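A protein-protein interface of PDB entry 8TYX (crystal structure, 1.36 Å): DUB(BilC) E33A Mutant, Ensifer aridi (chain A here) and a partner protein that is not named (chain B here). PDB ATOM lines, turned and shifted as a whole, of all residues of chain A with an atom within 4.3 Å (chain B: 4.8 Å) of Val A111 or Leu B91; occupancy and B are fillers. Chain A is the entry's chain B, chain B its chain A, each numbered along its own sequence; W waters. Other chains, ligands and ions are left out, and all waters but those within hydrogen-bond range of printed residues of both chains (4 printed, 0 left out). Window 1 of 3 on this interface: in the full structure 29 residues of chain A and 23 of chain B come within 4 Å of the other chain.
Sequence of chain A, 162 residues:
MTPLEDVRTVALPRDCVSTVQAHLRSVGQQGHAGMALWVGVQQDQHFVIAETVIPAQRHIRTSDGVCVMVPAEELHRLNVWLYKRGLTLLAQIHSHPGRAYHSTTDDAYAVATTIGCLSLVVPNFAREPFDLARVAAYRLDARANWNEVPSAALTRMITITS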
ATOM      1  N   MET A  35      23.441 -21.569  -1.592  1.00  0.00           N
ATOM      2  CA  MET A  35      22.591 -22.711  -1.283  1.00  0.00           C
ATOM      3  C   MET A  35      22.558 -23.679  -2.466  1.00  0.00           C
ATOM      4  O   MET A  35      22.501 -23.264  -3.628  1.00  0.00           O
ATOM      5  CB  MET A  35      21.140 -22.278  -0.959  1.00  0.00           C
ATOM      6  CG  MET A  35      20.257 -23.442  -0.481  1.00  0.00           C
ATOM      7  SD  MET A  35      18.499 -23.076  -0.256  1.00  0.00           S
ATOM      8  CE  MET A  35      18.583 -21.917   1.072  1.00  0.00           C
ATOM      9  N   LEU A  37      20.937 -27.988  -3.359  1.00  0.00           N
ATOM     10  CA  LEU A  37      19.959 -28.997  -2.972  1.00  0.00           C
ATOM     11  C   LEU A  37      20.366 -30.340  -3.561  1.00  0.00           C
ATOM     12  O   LEU A  37      20.833 -30.399  -4.698  1.00  0.00           O
ATOM     13  CB  LEU A  37      18.562 -28.642  -3.505  1.00  0.00           C
ATOM     14  CG  LEU A  37      18.000 -27.255  -3.148  1.00  0.00           C
ATOM     15  CD1 LEU A  37      16.732 -26.978  -3.949  1.00  0.00           C
ATOM     16  CD2 LEU A  37      17.738 -27.149  -1.647  1.00  0.00           C
ATOM     17  N   ALA A  72       9.880 -17.161  -4.405  1.00  0.00           N
ATOM     18  CA  ALA A  72       8.691 -17.983  -4.584  1.00  0.00           C
ATOM     19  C   ALA A  72       8.601 -18.602  -5.973  1.00  0.00           C
ATOM     20  O   ALA A  72       8.235 -19.777  -6.105  1.00  0.00           O
ATOM     21  CB  ALA A  72       7.439 -17.151  -4.305  1.00  0.00           C
ATOM     22  N   LEU A  75      10.772 -21.642  -6.058  1.00  0.00           N
ATOM     23  CA  LEU A  75      10.257 -22.745  -5.248  1.00  0.00           C
ATOM     24  C   LEU A  75       9.100 -23.443  -5.959  1.00  0.00           C
ATOM     25  O   LEU A  75       8.976 -24.673  -5.898  1.00  0.00           O
ATOM     26  CB  LEU A  75       9.869 -22.219  -3.871  1.00  0.00           C
ATOM     27  CG  LEU A  75      11.063 -21.676  -3.102  1.00  0.00           C
ATOM     28  CD1 LEU A  75      10.717 -20.649  -2.036  1.00  0.00           C
ATOM     29  CD2 LEU A  75      11.892 -22.806  -2.483  1.00  0.00           C
ATOM     30  N   LEU A  89      13.191 -34.418  -2.800  1.00  0.00           N
ATOM     31  CA  LEU A  89      14.144 -33.494  -2.203  1.00  0.00           C
ATOM     32  C   LEU A  89      14.609 -34.055  -0.857  1.00  0.00           C
ATOM     33  O   LEU A  89      13.821 -34.179   0.089  1.00  0.00           O
ATOM     34  CB  LEU A  89      13.520 -32.111  -2.059  1.00  0.00           C
ATOM     35  CG  LEU A  89      14.333 -31.093  -1.277  1.00  0.00           C
ATOM     36  CD1 LEU A  89      15.684 -30.790  -1.919  1.00  0.00           C
ATOM     37  CD2 LEU A  89      13.542 -29.797  -1.099  1.00  0.00           C
ATOM     38  N   GLN A  92      19.172 -29.827   1.841  1.00  0.00           N
ATOM     39  CA  GLN A  92      19.716 -28.536   1.480  1.00  0.00           C
ATOM     40  C   GLN A  92      21.120 -28.409   2.055  1.00  0.00           C
ATOM     41  O   GLN A  92      21.452 -29.022   3.073  1.00  0.00           O
ATOM     42  CB  GLN A  92      18.841 -27.386   1.954  1.00  0.00           C
ATOM     43  CG  GLN A  92      18.621 -27.332   3.446  1.00  0.00           C
ATOM     44  CD  GLN A  92      17.714 -26.182   3.835  1.00  0.00           C
ATOM     45  OE1 GLN A  92      16.643 -26.023   3.265  1.00  0.00           O
ATOM     46  NE2 GLN A  92      18.153 -25.370   4.810  1.00  0.00           N
ATOM     47  N   TYR A 109      13.393 -21.115   8.102  1.00  0.00           N
ATOM     48  CA  TYR A 109      13.017 -20.850   6.700  1.00  0.00           C
ATOM     49  C   TYR A 109      13.583 -21.881   5.724  1.00  0.00           C
ATOM     50  O   TYR A 109      13.904 -21.570   4.576  1.00  0.00           O
ATOM     51  CB  TYR A 109      13.409 -19.435   6.252  1.00  0.00           C
ATOM     52  CG  TYR A 109      12.855 -18.360   7.158  1.00  0.00           C
ATOM     53  CD1 TYR A 109      11.496 -18.119   7.266  1.00  0.00           C
ATOM     54  CD2 TYR A 109      13.712 -17.595   7.932  1.00  0.00           C
ATOM     55  CE1 TYR A 109      11.016 -17.123   8.127  1.00  0.00           C
ATOM     56  CE2 TYR A 109      13.249 -16.611   8.788  1.00  0.00           C
ATOM     57  CZ  TYR A 109      11.900 -16.376   8.871  1.00  0.00           C
ATOM     58  OH  TYR A 109      11.457 -15.391   9.731  1.00  0.00           O
ATOM     59  N   ALA A 110      13.672 -23.132   6.146  1.00  0.00           N
ATOM     60  CA  ALA A 110      14.263 -24.154   5.303  1.00  0.00           C
ATOM     61  C   ALA A 110      13.428 -24.440   4.048  1.00  0.00           C
ATOM     62  O   ALA A 110      12.195 -24.325   4.032  1.00  0.00           O
ATOM     63  CB  ALA A 110      14.482 -25.450   6.083  1.00  0.00           C
ATOM     64  N   VAL A 111      14.143 -24.834   2.981  1.00  0.00           N
ATOM     65  CA  VAL A 111      13.556 -25.313   1.732  1.00  0.00           C
ATOM     66  C   VAL A 111      13.294 -26.817   1.778  1.00  0.00           C
ATOM     67  O   VAL A 111      12.335 -27.313   1.178  1.00  0.00           O
ATOM     68  CB  VAL A 111      14.482 -24.935   0.553  1.00  0.00           C
ATOM     69  CG1 VAL A 111      14.033 -25.521  -0.782  1.00  0.00           C
ATOM     70  CG2 VAL A 111      14.639 -23.393   0.440  1.00  0.00           C
ATOM     71  N   ALA A 112      14.176 -27.581   2.425  1.00  0.00           N
ATOM     72  CA  ALA A 112      14.003 -29.046   2.559  1.00  0.00           C
ATOM     73  C   ALA A 112      13.101 -29.287   3.756  1.00  0.00           C
ATOM     74  O   ALA A 112      13.559 -29.353   4.894  1.00  0.00           O
ATOM     75  CB  ALA A 112      15.357 -29.727   2.707  1.00  0.00           C
ATOM     76  N   THR A 113      11.789 -29.340   3.496  1.00  0.00           N
ATOM     77  CA  THR A 113      10.778 -29.133   4.545  1.00  0.00           C
ATOM     78  C   THR A 113      10.179 -30.414   5.112  1.00  0.00           C
ATOM     79  O   THR A 113       9.401 -30.324   6.073  1.00  0.00           O
ATOM     80  CB  THR A 113       9.643 -28.275   3.994  1.00  0.00           C
ATOM     81  OG1 THR A 113       9.152 -28.883   2.804  1.00  0.00           O
ATOM     82  CG2 THR A 113      10.054 -26.853   3.673  1.00  0.00           C
ATOM     83  N   ASN B  25       6.674 -30.391  -2.876  1.00  0.00           N
ATOM     84  CA  ASN B  25       8.020 -30.877  -3.178  1.00  0.00           C
ATOM     85  C   ASN B  25       7.976 -32.105  -4.086  1.00  0.00           C
ATOM     86  O   ASN B  25       8.662 -33.103  -3.866  1.00  0.00           O
ATOM     87  CB  ASN B  25       8.836 -31.172  -1.903  1.00  0.00           C
ATOM     88  CG  ASN B  25       9.124 -29.954  -1.097  1.00  0.00           C
ATOM     89  OD1 ASN B  25       8.963 -29.952   0.133  1.00  0.00           O
ATOM     90  ND2 ASN B  25       9.565 -28.909  -1.768  1.00  0.00           N
ATOM     91  N   GLN B  55       8.199 -25.327   7.713  1.00  0.00           N
ATOM     92  CA  GLN B  55       7.574 -24.021   7.810  1.00  0.00           C
ATOM     93  C   GLN B  55       6.078 -24.244   7.962  1.00  0.00           C
ATOM     94  O   GLN B  55       5.533 -25.209   7.391  1.00  0.00           O
ATOM     95  CB  GLN B  55       7.850 -23.168   6.568  1.00  0.00           C
ATOM     96  CG  GLN B  55       9.321 -22.827   6.385  1.00  0.00           C
ATOM     97  CD  GLN B  55       9.548 -21.713   5.371  1.00  0.00           C
ATOM     98  OE1 GLN B  55       8.825 -20.709   5.368  1.00  0.00           O
ATOM     99  NE2 GLN B  55      10.536 -21.871   4.512  1.00  0.00           N
ATOM    100  N   ASN B  59       2.905 -20.295   5.483  1.00  0.00           N
ATOM    101  CA  ASN B  59       4.115 -19.964   4.743  1.00  0.00           C
ATOM    102  C   ASN B  59       4.152 -20.598   3.360  1.00  0.00           C
ATOM    103  O   ASN B  59       5.170 -20.505   2.668  1.00  0.00           O
ATOM    104  CB  ASN B  59       5.340 -20.383   5.558  1.00  0.00           C
ATOM    105  CG  ASN B  59       5.658 -19.405   6.652  1.00  0.00           C
ATOM    106  OD1 ASN B  59       4.803 -18.620   7.066  1.00  0.00           O
ATOM    107  ND2 ASN B  59       6.906 -19.398   7.108  1.00  0.00           N
ATOM    108  N   TRP B  60       3.019 -21.145   2.909  1.00  0.00           N
ATOM    109  CA  TRP B  60       2.907 -21.843   1.639  1.00  0.00           C
ATOM    110  C   TRP B  60       1.758 -21.250   0.832  1.00  0.00           C
ATOM    111  O   TRP B  60       0.778 -20.732   1.387  1.00  0.00           O
ATOM    112  CB  TRP B  60       2.617 -23.343   1.857  1.00  0.00           C
ATOM    113  CG  TRP B  60       3.622 -24.104   2.671  1.00  0.00           C
ATOM    114  CD1 TRP B  60       3.792 -24.030   4.016  1.00  0.00           C
ATOM    115  CD2 TRP B  60       4.553 -25.084   2.194  1.00  0.00           C
ATOM    116  NE1 TRP B  60       4.778 -24.901   4.409  1.00  0.00           N
ATOM    117  CE2 TRP B  60       5.264 -25.549   3.302  1.00  0.00           C
ATOM    118  CE3 TRP B  60       4.854 -25.601   0.938  1.00  0.00           C
ATOM    119  CZ2 TRP B  60       6.248 -26.530   3.193  1.00  0.00           C
ATOM    120  CZ3 TRP B  60       5.850 -26.559   0.828  1.00  0.00           C
ATOM    121  CH2 TRP B  60       6.542 -27.005   1.935  1.00  0.00           C
ATOM    122  N   LEU B  89       1.542 -26.729  -4.306  1.00  0.00           N
ATOM    123  CA  LEU B  89       1.625 -26.012  -3.058  1.00  0.00           C
ATOM    124  C   LEU B  89       3.108 -25.854  -2.746  1.00  0.00           C
ATOM    125  O   LEU B  89       3.835 -26.854  -2.590  1.00  0.00           O
ATOM    126  CB  LEU B  89       0.961 -26.798  -1.922  1.00  0.00           C
ATOM    127  CG  LEU B  89       0.917 -26.169  -0.526  1.00  0.00           C
ATOM    128  CD1 LEU B  89       0.150 -24.846  -0.583  1.00  0.00           C
ATOM    129  CD2 LEU B  89       0.282 -27.112   0.486  1.00  0.00           C
ATOM    130  N   SER B  90       3.568 -24.604  -2.685  1.00  0.00           N
ATOM    131  CA  SER B  90       4.989 -24.320  -2.575  1.00  0.00           C
ATOM    132  C   SER B  90       5.253 -23.184  -1.600  1.00  0.00           C
ATOM    133  O   SER B  90       4.375 -22.380  -1.303  1.00  0.00           O
ATOM    134  CB  SER B  90       5.590 -23.939  -3.942  1.00  0.00           C
ATOM    135  OG  SER B  90       5.102 -24.768  -4.997  1.00  0.00           O
ATOM    136  N   LEU B  91       6.489 -23.115  -1.130  1.00  0.00           N
ATOM    137  CA  LEU B  91       6.856 -22.126  -0.147  1.00  0.00           C
ATOM    138  C   LEU B  91       6.837 -20.709  -0.726  1.00  0.00           C
ATOM    139  O   LEU B  91       7.199 -20.470  -1.884  1.00  0.00           O
ATOM    140  CB  LEU B  91       8.287 -22.385   0.325  1.00  0.00           C
ATOM    141  CG  LEU B  91       8.471 -23.522   1.310  1.00  0.00           C
ATOM    142  CD1 LEU B  91       9.947 -23.803   1.525  1.00  0.00           C
ATOM    143  CD2 LEU B  91       7.768 -23.219   2.637  1.00  0.00           C
ATOM    144  N   LYS B  92       6.449 -19.761   0.131  1.00  0.00           N
ATOM    145  CA  LYS B  92       6.571 -18.349  -0.210  1.00  0.00           C
ATOM    146  C   LYS B  92       8.016 -17.862  -0.204  1.00  0.00           C
ATOM    147  O   LYS B  92       8.360 -16.950  -0.972  1.00  0.00           O
ATOM    148  CB  LYS B  92       5.754 -17.515   0.773  1.00  0.00           C
ATOM    149  CG  LYS B  92       4.256 -17.784   0.673  1.00  0.00           C
ATOM    150  CD  LYS B  92       3.486 -17.058   1.770  1.00  0.00           C
ATOM    151  CE  LYS B  92       2.006 -17.376   1.705  1.00  0.00           C
ATOM    152  NZ  LYS B  92       1.278 -16.751   2.819  1.00  0.00           N
ATOM    153  N   ALA B  93       8.865 -18.434   0.643  1.00  0.00           N
ATOM    154  CA  ALA B  93      10.249 -18.013   0.752  1.00  0.00           C
ATOM    155  C   ALA B  93      11.084 -19.113   1.381  1.00  0.00           C
ATOM    156  O   ALA B  93      10.591 -19.869   2.215  1.00  0.00           O
ATOM    157  CB  ALA B  93      10.363 -16.759   1.621  1.00  0.00           C
ATOM    158  N   GLY B  94      12.340 -19.187   0.963  1.00  0.00           N
ATOM    159  CA  GLY B  94      13.333 -20.037   1.574  1.00  0.00           C
ATOM    160  C   GLY B  94      14.556 -19.193   1.886  1.00  0.00           C
ATOM    161  O   GLY B  94      15.015 -18.430   1.019  1.00  0.00           O
HETATM  162  O   HOH W   1       6.312 -20.713  -4.348  1.00  0.00           O
HETATM  163  O   HOH W   2      10.444 -34.252  -2.190  1.00  0.00           O
HETATM  164  O   HOH W   3       9.831 -26.791  -0.021  1.00  0.00           O
HETATM  165  O   HOH W   4      10.151 -15.035  -1.657  1.00  0.00           O
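OD1 of Asn B25 lies within hydrogen-bond range of OG1 of Thr A113 (2.9 Å).
O of Tyr A109 sits close to NE2 of Gln B55 (3.4 Å).
NE2 of Gln B55 sits at hydrogen-bond distance from O of Ala A110, 3.0 Å away.
The side-chain amide oxygen (OE1) of Gln B55 sits at hydrogen-bond distance from the side-chain amide nitrogen (ND2) of Asn B59 (2.9 Å).
O of Gln B55 is in hydrogen-bond range of NE1 of Trp B60, 3.1 Å away.
The side-chain amide nitrogen (NE2) of Gln B55 lies within hydrogen-bond range of the backbone carbonyl oxygen (O) of Ala B93.
O of Asn B59 lies within hydrogen-bond range of N of Lys B92, 2.9 Å away.
The backbone NH of Val A111 sits at hydrogen-bond distance from the side-chain amide oxygen of Gln A92, 2.8 Å away.
Among the printed residues, pairs that only touch across the chains: Ala A72 with Leu B91 (3.96 Å), Ala A72 with Lys B92 (3.5 Å), Leu A75 with Ser B90 (3.98 Å), Leu A75 with Leu B91 (3.5 Å), Leu A75 with Ala B93 (3.8 Å), Leu A75 with Gly B94 (3.7 Å), Tyr A109 with Gly B94 (3.4 Å), Ala A110 with Leu B91 (3.4 Å), Val A111 with Leu B91 (3.9 Å), Val A111 with Gly B94 (3.8 Å), Thr A113 with Trp B60 (3.3 Å) and Thr A113 with Leu B91 (3.7 Å).
Leu B91 touches just these residues of chain A: Ala A72, Leu A75, Ala A110, Val A111 and Thr A113.
Printed residues of chain A within 4 Å of Lys B92: Ala A72 (3.5 Å).
Of the printed residues of chain B, Ala A72 touches Leu B91 and Lys B92.
Of the printed residues of chain A, Gln B55 touches Tyr A109 and Ala A110.
Of the printed residues of chain B, Ala A110 touches Gln B55 (3.0 Å) and Leu B91 (3.4 Å).
Of the printed residues of chain A, Ser B90 touches Leu A75 (3.98 Å).
Ala A112 touches none of the printed residues of chain B.
The nearest residue of chain B that does not touch Val A111 is Asn B25 (4.3 Å).
Along chain B the printed residues that touch a printed residue of chain A span positions 25 to 94.
Of the 11 printed residues of chain A, 6 touch a printed residue of chain B.
Among the printed residues, 15 pairs touch across the chains.
Water W1 bridges the backbone carbonyl oxygen of Leu B91 (2.6 Å) and the backbone carbonyl oxygen of Ala A72 (2.8 Å).
Water W2 lies within hydrogen-bond range of the backbone carbonyl oxygen (O) of Asn B25 (2.7 Å) and the backbone NH (N) of Leu A89 (2.8 Å).
Water W4 lies within hydrogen-bond range of the backbone carbonyl oxygen of Lys B92 (2.7 Å) and the backbone NH of Ala A72 (3.5 Å).
Water W3 lies within hydrogen-bond range of ND2 of Asn B25 (2.8 Å) and O of Val A111 (2.8 Å).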
